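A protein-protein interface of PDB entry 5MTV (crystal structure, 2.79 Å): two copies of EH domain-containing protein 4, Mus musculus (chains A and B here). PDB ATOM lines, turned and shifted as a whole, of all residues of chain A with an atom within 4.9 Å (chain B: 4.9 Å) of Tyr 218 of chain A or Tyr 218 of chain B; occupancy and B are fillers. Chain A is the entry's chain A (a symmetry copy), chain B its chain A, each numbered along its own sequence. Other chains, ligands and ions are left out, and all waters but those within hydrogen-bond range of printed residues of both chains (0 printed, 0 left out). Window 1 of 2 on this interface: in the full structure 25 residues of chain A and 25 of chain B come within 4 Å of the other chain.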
ATOM      1  N   LEU A 203       9.077 -19.784  11.308  1.00  0.00           N
ATOM      2  CA  LEU A 203       8.980 -18.409  10.827  1.00  0.00           C
ATOM      3  C   LEU A 203       7.624 -17.877  11.270  1.00  0.00           C
ATOM      4  O   LEU A 203       6.589 -18.208  10.686  1.00  0.00           O
ATOM      5  CB  LEU A 203       9.159 -18.346   9.314  1.00  0.00           C
ATOM      6  CG  LEU A 203       9.067 -16.954   8.686  1.00  0.00           C
ATOM      7  CD1 LEU A 203       9.979 -15.952   9.391  1.00  0.00           C
ATOM      8  CD2 LEU A 203       9.411 -17.037   7.210  1.00  0.00           C
ATOM      9  N   GLN A 213       7.125  -9.636   0.705  1.00  0.00           N
ATOM     10  CA  GLN A 213       8.051  -9.460   1.818  1.00  0.00           C
ATOM     11  C   GLN A 213       8.268 -10.765   2.567  1.00  0.00           C
ATOM     12  O   GLN A 213       9.353 -10.995   3.111  1.00  0.00           O
ATOM     13  CB  GLN A 213       7.534  -8.382   2.771  1.00  0.00           C
ATOM     14  CG  GLN A 213       8.503  -8.029   3.896  1.00  0.00           C
ATOM     15  CD  GLN A 213       9.859  -7.561   3.392  1.00  0.00           C
ATOM     16  OE1 GLN A 213      10.887  -7.832   4.014  1.00  0.00           O
ATOM     17  NE2 GLN A 213       9.871  -6.850   2.265  1.00  0.00           N
ATOM     18  N   LEU A 214       7.254 -11.629   2.609  1.00  0.00           N
ATOM     19  CA  LEU A 214       7.428 -12.932   3.239  1.00  0.00           C
ATOM     20  C   LEU A 214       8.479 -13.754   2.504  1.00  0.00           C
ATOM     21  O   LEU A 214       9.280 -14.456   3.130  1.00  0.00           O
ATOM     22  CB  LEU A 214       6.092 -13.676   3.280  1.00  0.00           C
ATOM     23  CG  LEU A 214       6.125 -15.095   3.855  1.00  0.00           C
ATOM     24  CD1 LEU A 214       6.687 -15.098   5.270  1.00  0.00           C
ATOM     25  CD2 LEU A 214       4.738 -15.713   3.829  1.00  0.00           C
ATOM     26  N   MET A 215       8.492 -13.678   1.172  1.00  0.00           N
ATOM     27  CA  MET A 215       9.497 -14.403   0.403  1.00  0.00           C
ATOM     28  C   MET A 215      10.869 -13.761   0.542  1.00  0.00           C
ATOM     29  O   MET A 215      11.889 -14.454   0.457  1.00  0.00           O
ATOM     30  CB  MET A 215       9.085 -14.464  -1.070  1.00  0.00           C
ATOM     31  CG  MET A 215       7.665 -14.954  -1.293  1.00  0.00           C
ATOM     32  SD  MET A 215       7.339 -16.543  -0.508  1.00  0.00           S
ATOM     33  CE  MET A 215       8.274 -17.627  -1.575  1.00  0.00           C
ATOM     34  N   ARG A 216      10.916 -12.445   0.753  1.00  0.00           N
ATOM     35  CA  ARG A 216      12.191 -11.776   0.986  1.00  0.00           C
ATOM     36  C   ARG A 216      12.771 -12.174   2.335  1.00  0.00           C
ATOM     37  O   ARG A 216      13.946 -12.544   2.435  1.00  0.00           O
ATOM     38  CB  ARG A 216      12.012 -10.259   0.911  1.00  0.00           C
ATOM     39  CG  ARG A 216      12.617  -9.613  -0.325  1.00  0.00           C
ATOM     40  CD  ARG A 216      11.790  -9.887  -1.565  1.00  0.00           C
ATOM     41  NE  ARG A 216      12.135 -11.155  -2.196  1.00  0.00           N
ATOM     42  CZ  ARG A 216      11.388 -11.759  -3.112  1.00  0.00           C
ATOM     43  NH1 ARG A 216      10.241 -11.218  -3.500  1.00  0.00           N
ATOM     44  NH2 ARG A 216      11.780 -12.910  -3.636  1.00  0.00           N
ATOM     45  N   VAL A 217      11.957 -12.101   3.389  1.00  0.00           N
ATOM     46  CA  VAL A 217      12.427 -12.447   4.726  1.00  0.00           C
ATOM     47  C   VAL A 217      12.765 -13.929   4.801  1.00  0.00           C
ATOM     48  O   VAL A 217      13.850 -14.316   5.249  1.00  0.00           O
ATOM     49  CB  VAL A 217      11.373 -12.054   5.776  1.00  0.00           C
ATOM     50  CG1 VAL A 217      11.797 -12.508   7.159  1.00  0.00           C
ATOM     51  CG2 VAL A 217      11.148 -10.547   5.765  1.00  0.00           C
ATOM     52  N   TYR A 218      11.833 -14.783   4.372  1.00  0.00           N
ATOM     53  CA  TYR A 218      12.081 -16.220   4.382  1.00  0.00           C
ATOM     54  C   TYR A 218      13.350 -16.562   3.612  1.00  0.00           C
ATOM     55  O   TYR A 218      14.123 -17.432   4.030  1.00  0.00           O
ATOM     56  CB  TYR A 218      10.871 -16.952   3.801  1.00  0.00           C
ATOM     57  CG  TYR A 218      11.040 -18.448   3.664  1.00  0.00           C
ATOM     58  CD1 TYR A 218      11.491 -19.219   4.726  1.00  0.00           C
ATOM     59  CD2 TYR A 218      10.728 -19.092   2.476  1.00  0.00           C
ATOM     60  CE1 TYR A 218      11.639 -20.588   4.601  1.00  0.00           C
ATOM     61  CE2 TYR A 218      10.870 -20.458   2.343  1.00  0.00           C
ATOM     62  CZ  TYR A 218      11.325 -21.203   3.406  1.00  0.00           C
ATOM     63  OH  TYR A 218      11.463 -22.565   3.268  1.00  0.00           O
ATOM     64  N   GLY A 219      13.589 -15.880   2.493  1.00  0.00           N
ATOM     65  CA  GLY A 219      14.808 -16.125   1.742  1.00  0.00           C
ATOM     66  C   GLY A 219      16.050 -15.705   2.505  1.00  0.00           C
ATOM     67  O   GLY A 219      17.060 -16.414   2.503  1.00  0.00           O
ATOM     68  N   ALA A 220      15.992 -14.548   3.170  1.00  0.00           N
ATOM     69  CA  ALA A 220      17.123 -14.095   3.973  1.00  0.00           C
ATOM     70  C   ALA A 220      17.392 -15.050   5.127  1.00  0.00           C
ATOM     71  O   ALA A 220      18.552 -15.333   5.452  1.00  0.00           O
ATOM     72  CB  ALA A 220      16.859 -12.685   4.498  1.00  0.00           C
ATOM     73  N   LEU A 221      16.333 -15.559   5.757  1.00  0.00           N
ATOM     74  CA  LEU A 221      16.499 -16.486   6.872  1.00  0.00           C
ATOM     75  C   LEU A 221      17.286 -17.718   6.446  1.00  0.00           C
ATOM     76  O   LEU A 221      18.263 -18.102   7.099  1.00  0.00           O
ATOM     77  CB  LEU A 221      15.127 -16.884   7.421  1.00  0.00           C
ATOM     78  CG  LEU A 221      15.109 -17.984   8.485  1.00  0.00           C
ATOM     79  CD1 LEU A 221      15.986 -17.607   9.672  1.00  0.00           C
ATOM     80  CD2 LEU A 221      13.683 -18.261   8.935  1.00  0.00           C
ATOM     81  N   MET A 222      16.872 -18.355   5.349  1.00  0.00           N
ATOM     82  CA  MET A 222      17.565 -19.547   4.877  1.00  0.00           C
ATOM     83  C   MET A 222      18.940 -19.209   4.317  1.00  0.00           C
ATOM     84  O   MET A 222      19.874 -20.009   4.439  1.00  0.00           O
ATOM     85  CB  MET A 222      16.720 -20.255   3.819  1.00  0.00           C
ATOM     86  CG  MET A 222      15.347 -20.655   4.317  1.00  0.00           C
ATOM     87  SD  MET A 222      15.438 -21.924   5.587  1.00  0.00           S
ATOM     88  CE  MET A 222      15.671 -23.388   4.585  1.00  0.00           C
ATOM     89  N   VAL A 237      11.728 -25.343   7.872  1.00  0.00           N
ATOM     90  CA  VAL A 237      11.129 -24.142   8.440  1.00  0.00           C
ATOM     91  C   VAL A 237       9.618 -24.308   8.389  1.00  0.00           C
ATOM     92  O   VAL A 237       9.064 -24.699   7.354  1.00  0.00           O
ATOM     93  CB  VAL A 237      11.560 -22.873   7.685  1.00  0.00           C
ATOM     94  CG1 VAL A 237      10.913 -21.637   8.302  1.00  0.00           C
ATOM     95  CG2 VAL A 237      13.068 -22.730   7.688  1.00  0.00           C
ATOM     96  N   ILE A 239       6.355 -22.145   8.450  1.00  0.00           N
ATOM     97  CA  ILE A 239       5.936 -20.768   8.209  1.00  0.00           C
ATOM     98  C   ILE A 239       4.482 -20.623   8.629  1.00  0.00           C
ATOM     99  O   ILE A 239       3.619 -21.389   8.180  1.00  0.00           O
ATOM    100  CB  ILE A 239       6.115 -20.381   6.731  1.00  0.00           C
ATOM    101  CG1 ILE A 239       7.574 -20.553   6.301  1.00  0.00           C
ATOM    102  CG2 ILE A 239       5.662 -18.941   6.495  1.00  0.00           C
ATOM    103  CD1 ILE A 239       7.786 -20.438   4.803  1.00  0.00           C
ATOM    104  N   LEU B 203      13.580 -18.132  -9.868  1.00  0.00           N
ATOM    105  CA  LEU B 203      13.020 -19.435  -9.521  1.00  0.00           C
ATOM    106  C   LEU B 203      11.863 -19.691 -10.477  1.00  0.00           C
ATOM    107  O   LEU B 203      10.776 -19.128 -10.326  1.00  0.00           O
ATOM    108  CB  LEU B 203      12.582 -19.470  -8.061  1.00  0.00           C
ATOM    109  CG  LEU B 203      11.966 -20.784  -7.577  1.00  0.00           C
ATOM    110  CD1 LEU B 203      12.850 -21.982  -7.916  1.00  0.00           C
ATOM    111  CD2 LEU B 203      11.721 -20.711  -6.081  1.00  0.00           C
ATOM    112  N   GLN B 213       5.609 -27.193  -1.290  1.00  0.00           N
ATOM    113  CA  GLN B 213       6.835 -27.604  -1.963  1.00  0.00           C
ATOM    114  C   GLN B 213       7.591 -26.406  -2.514  1.00  0.00           C
ATOM    115  O   GLN B 213       8.824 -26.430  -2.585  1.00  0.00           O
ATOM    116  CB  GLN B 213       6.516 -28.591  -3.087  1.00  0.00           C
ATOM    117  CG  GLN B 213       7.748 -29.185  -3.763  1.00  0.00           C
ATOM    118  CD  GLN B 213       8.674 -29.903  -2.793  1.00  0.00           C
ATOM    119  OE1 GLN B 213       9.894 -29.878  -2.956  1.00  0.00           O
ATOM    120  NE2 GLN B 213       8.100 -30.552  -1.781  1.00  0.00           N
ATOM    121  N   LEU B 214       6.876 -25.353  -2.909  1.00  0.00           N
ATOM    122  CA  LEU B 214       7.548 -24.142  -3.366  1.00  0.00           C
ATOM    123  C   LEU B 214       8.378 -23.526  -2.247  1.00  0.00           C
ATOM    124  O   LEU B 214       9.486 -23.033  -2.484  1.00  0.00           O
ATOM    125  CB  LEU B 214       6.518 -23.139  -3.891  1.00  0.00           C
ATOM    126  CG  LEU B 214       7.066 -21.784  -4.346  1.00  0.00           C
ATOM    127  CD1 LEU B 214       8.119 -21.957  -5.432  1.00  0.00           C
ATOM    128  CD2 LEU B 214       5.938 -20.890  -4.834  1.00  0.00           C
ATOM    129  N   MET B 215       7.858 -23.546  -1.019  1.00  0.00           N
ATOM    130  CA  MET B 215       8.613 -23.015   0.110  1.00  0.00           C
ATOM    131  C   MET B 215       9.766 -23.933   0.486  1.00  0.00           C
ATOM    132  O   MET B 215      10.794 -23.465   0.988  1.00  0.00           O
ATOM    133  CB  MET B 215       7.686 -22.806   1.309  1.00  0.00           C
ATOM    134  CG  MET B 215       6.425 -22.023   0.985  1.00  0.00           C
ATOM    135  SD  MET B 215       6.767 -20.436   0.203  1.00  0.00           S
ATOM    136  CE  MET B 215       7.419 -19.526   1.594  1.00  0.00           C
ATOM    137  N   ARG B 216       9.616 -25.238   0.254  1.00  0.00           N
ATOM    138  CA  ARG B 216      10.712 -26.167   0.504  1.00  0.00           C
ATOM    139  C   ARG B 216      11.839 -25.956  -0.497  1.00  0.00           C
ATOM    140  O   ARG B 216      13.010 -25.843  -0.118  1.00  0.00           O
ATOM    141  CB  ARG B 216      10.208 -27.609   0.440  1.00  0.00           C
ATOM    142  CG  ARG B 216      10.138 -28.313   1.785  1.00  0.00           C
ATOM    143  CD  ARG B 216       8.971 -27.821   2.618  1.00  0.00           C
ATOM    144  NE  ARG B 216       9.301 -26.627   3.387  1.00  0.00           N
ATOM    145  CZ  ARG B 216       8.400 -25.842   3.967  1.00  0.00           C
ATOM    146  NH1 ARG B 216       7.107 -26.116   3.857  1.00  0.00           N
ATOM    147  NH2 ARG B 216       8.789 -24.777   4.651  1.00  0.00           N
ATOM    148  N   VAL B 217      11.500 -25.903  -1.785  1.00  0.00           N
ATOM    149  CA  VAL B 217      12.513 -25.719  -2.819  1.00  0.00           C
ATOM    150  C   VAL B 217      13.154 -24.344  -2.695  1.00  0.00           C
ATOM    151  O   VAL B 217      14.382 -24.211  -2.671  1.00  0.00           O
ATOM    152  CB  VAL B 217      11.891 -25.928  -4.211  1.00  0.00           C
ATOM    153  CG1 VAL B 217      12.902 -25.631  -5.302  1.00  0.00           C
ATOM    154  CG2 VAL B 217      11.372 -27.353  -4.352  1.00  0.00           C
ATOM    155  N   TYR B 218      12.328 -23.298  -2.625  1.00  0.00           N
ATOM    156  CA  TYR B 218      12.854 -21.946  -2.477  1.00  0.00           C
ATOM    157  C   TYR B 218      13.766 -21.842  -1.262  1.00  0.00           C
ATOM    158  O   TYR B 218      14.803 -21.171  -1.310  1.00  0.00           O
ATOM    159  CB  TYR B 218      11.694 -20.954  -2.379  1.00  0.00           C
ATOM    160  CG  TYR B 218      12.104 -19.521  -2.124  1.00  0.00           C
ATOM    161  CD1 TYR B 218      13.081 -18.907  -2.895  1.00  0.00           C
ATOM    162  CD2 TYR B 218      11.497 -18.776  -1.124  1.00  0.00           C
ATOM    163  CE1 TYR B 218      13.450 -17.594  -2.664  1.00  0.00           C
ATOM    164  CE2 TYR B 218      11.858 -17.466  -0.888  1.00  0.00           C
ATOM    165  CZ  TYR B 218      12.832 -16.877  -1.660  1.00  0.00           C
ATOM    166  OH  TYR B 218      13.187 -15.569  -1.421  1.00  0.00           O
ATOM    167  N   GLY B 219      13.405 -22.511  -0.167  1.00  0.00           N
ATOM    168  CA  GLY B 219      14.260 -22.494   1.007  1.00  0.00           C
ATOM    169  C   GLY B 219      15.584 -23.194   0.767  1.00  0.00           C
ATOM    170  O   GLY B 219      16.638 -22.711   1.190  1.00  0.00           O
ATOM    171  N   ALA B 220      15.549 -24.341   0.084  1.00  0.00           N
ATOM    172  CA  ALA B 220      16.782 -25.053  -0.237  1.00  0.00           C
ATOM    173  C   ALA B 220      17.669 -24.225  -1.155  1.00  0.00           C
ATOM    174  O   ALA B 220      18.896 -24.203  -0.993  1.00  0.00           O
ATOM    175  CB  ALA B 220      16.455 -26.399  -0.883  1.00  0.00           C
ATOM    176  N   LEU B 221      17.068 -23.534  -2.125  1.00  0.00           N
ATOM    177  CA  LEU B 221      17.841 -22.710  -3.048  1.00  0.00           C
ATOM    178  C   LEU B 221      18.640 -21.652  -2.298  1.00  0.00           C
ATOM    179  O   LEU B 221      19.850 -21.507  -2.505  1.00  0.00           O
ATOM    180  CB  LEU B 221      16.905 -22.059  -4.067  1.00  0.00           C
ATOM    181  CG  LEU B 221      17.529 -21.025  -5.008  1.00  0.00           C
ATOM    182  CD1 LEU B 221      18.698 -21.626  -5.777  1.00  0.00           C
ATOM    183  CD2 LEU B 221      16.481 -20.477  -5.962  1.00  0.00           C
ATOM    184  N   MET B 222      17.975 -20.896  -1.421  1.00  0.00           N
ATOM    185  CA  MET B 222      18.663 -19.855  -0.667  1.00  0.00           C
ATOM    186  C   MET B 222      19.610 -20.448   0.367  1.00  0.00           C
ATOM    187  O   MET B 222      20.663 -19.865   0.650  1.00  0.00           O
ATOM    188  CB  MET B 222      17.642 -18.943   0.010  1.00  0.00           C
ATOM    189  CG  MET B 222      16.684 -18.288  -0.964  1.00  0.00           C
ATOM    190  SD  MET B 222      17.522 -17.120  -2.044  1.00  0.00           S
ATOM    191  CE  MET B 222      17.647 -15.696  -0.969  1.00  0.00           C
ATOM    192  N   VAL B 237      15.785 -13.105  -5.441  1.00  0.00           N
ATOM    193  CA  VAL B 237      15.218 -14.178  -6.246  1.00  0.00           C
ATOM    194  C   VAL B 237      13.876 -13.699  -6.777  1.00  0.00           C
ATOM    195  O   VAL B 237      13.059 -13.159  -6.023  1.00  0.00           O
ATOM    196  CB  VAL B 237      15.049 -15.476  -5.438  1.00  0.00           C
ATOM    197  CG1 VAL B 237      14.450 -16.575  -6.310  1.00  0.00           C
ATOM    198  CG2 VAL B 237      16.375 -15.929  -4.863  1.00  0.00           C
ATOM    199  N   ILE B 239      10.518 -15.137  -8.190  1.00  0.00           N
ATOM    200  CA  ILE B 239       9.763 -16.385  -8.189  1.00  0.00           C
ATOM    201  C   ILE B 239       8.589 -16.242  -9.145  1.00  0.00           C
ATOM    202  O   ILE B 239       7.800 -15.296  -9.033  1.00  0.00           O
ATOM    203  CB  ILE B 239       9.271 -16.738  -6.775  1.00  0.00           C
ATOM    204  CG1 ILE B 239      10.450 -16.855  -5.806  1.00  0.00           C
ATOM    205  CG2 ILE B 239       8.473 -18.041  -6.793  1.00  0.00           C
ATOM    206  CD1 ILE B 239      10.036 -16.948  -4.349  1.00  0.00           C
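O of Met 215 of chain B is in hydrogen-bond range of OH of Tyr 218 of chain A (2.5 Å). NH2 of Arg 216 of chain B is in hydrogen-bond range of O of Val 237 of chain A, at 2.7 Å. The backbone carbonyl oxygen of Met 215 of chain A is in hydrogen-bond range of the side-chain hydroxyl of Tyr 218 of chain B (2.5 Å). NH2 of Arg 216 of chain A lies within hydrogen-bond range of O of Val 237 of chain B (2.7 Å).
Among the printed residues, pairs that only touch across the chains: Met 215 of chain A with Ile 239 of chain B (3.4 Å), Ile 239 of chain A with Met 215 of chain B (3.4 Å), Gly 219 of chain A with Met 222 of chain B (3.6 Å), Met 222 of chain A with Gly 219 of chain B (3.6 Å), Tyr 218 of chain A with Gly 219 of chain B (3.6 Å), Gly 219 of chain A with Tyr 218 of chain B (3.6 Å), Met 215 of chain A with Met 215 of chain B (3.7 Å), Tyr 218 of chain A with Tyr 218 of chain B (3.7 Å), Tyr 218 of chain A with Arg 216 of chain B (3.7 Å), Arg 216 of chain A with Tyr 218 of chain B (3.7 Å) and Met 222 of chain A with Met 222 of chain B (3.9 Å).
Val 217 of chain A touches none of the printed residues of chain B. Of chain B, only Met 215, Arg 216, Tyr 218 and Gly 219 come within 4 Å of Tyr 218 of chain A. Printed residues of chain B within 4 Å of Val 237 of chain A: Arg 216 (2.7 Å). Gln 213 of chain B touches none of the printed residues of chain A. Printed residues of chain A within 4 Å of Met 215 of chain B: Met 215, Tyr 218 and Ile 239. Tyr 218 of chain B touches just these residues of chain A: Met 215, Arg 216, Tyr 218 and Gly 219. The nearest printed residue of chain B that does not touch Tyr 218 of chain A is Ala 220 of chain B (5.5 Å). The nearest printed residue of chain A that does not touch Tyr 218 of chain B is Ala 220 of chain A (5.5 Å).
Of the 13 printed residues of chain A, 7 touch a printed residue of chain B. Printed residues of chain A that touch a printed residue of chain B: Met 215, Arg 216, Tyr 218, Gly 219, Met 222, Val 237 and Ile 239. Hydrophobic or aromatic side chains of chain A within 4 Å of the printed part of chain B: Met 215, Tyr 218, Met 222 and Ile 239. Hydrophobic or aromatic side chains of chain B within 4 Å of the printed part of chain A: Met 215, Tyr 218, Met 222 and Ile 239. Among the printed residues, 15 pairs touch across the chains.
Met 215 of chain B touches its own counterpart, Met 215 of chain A. Tyr 218 of chain B touches its own counterpart, Tyr 218 of chain A. Gly 219 of chain A touches Met 222 of chain B, and with the chains exchanged Met 222 of chain A touches Gly 219 of chain B. Met 222 of chain A touches its own counterpart, Met 222 of chain B. 13 positions are printed for both chains.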
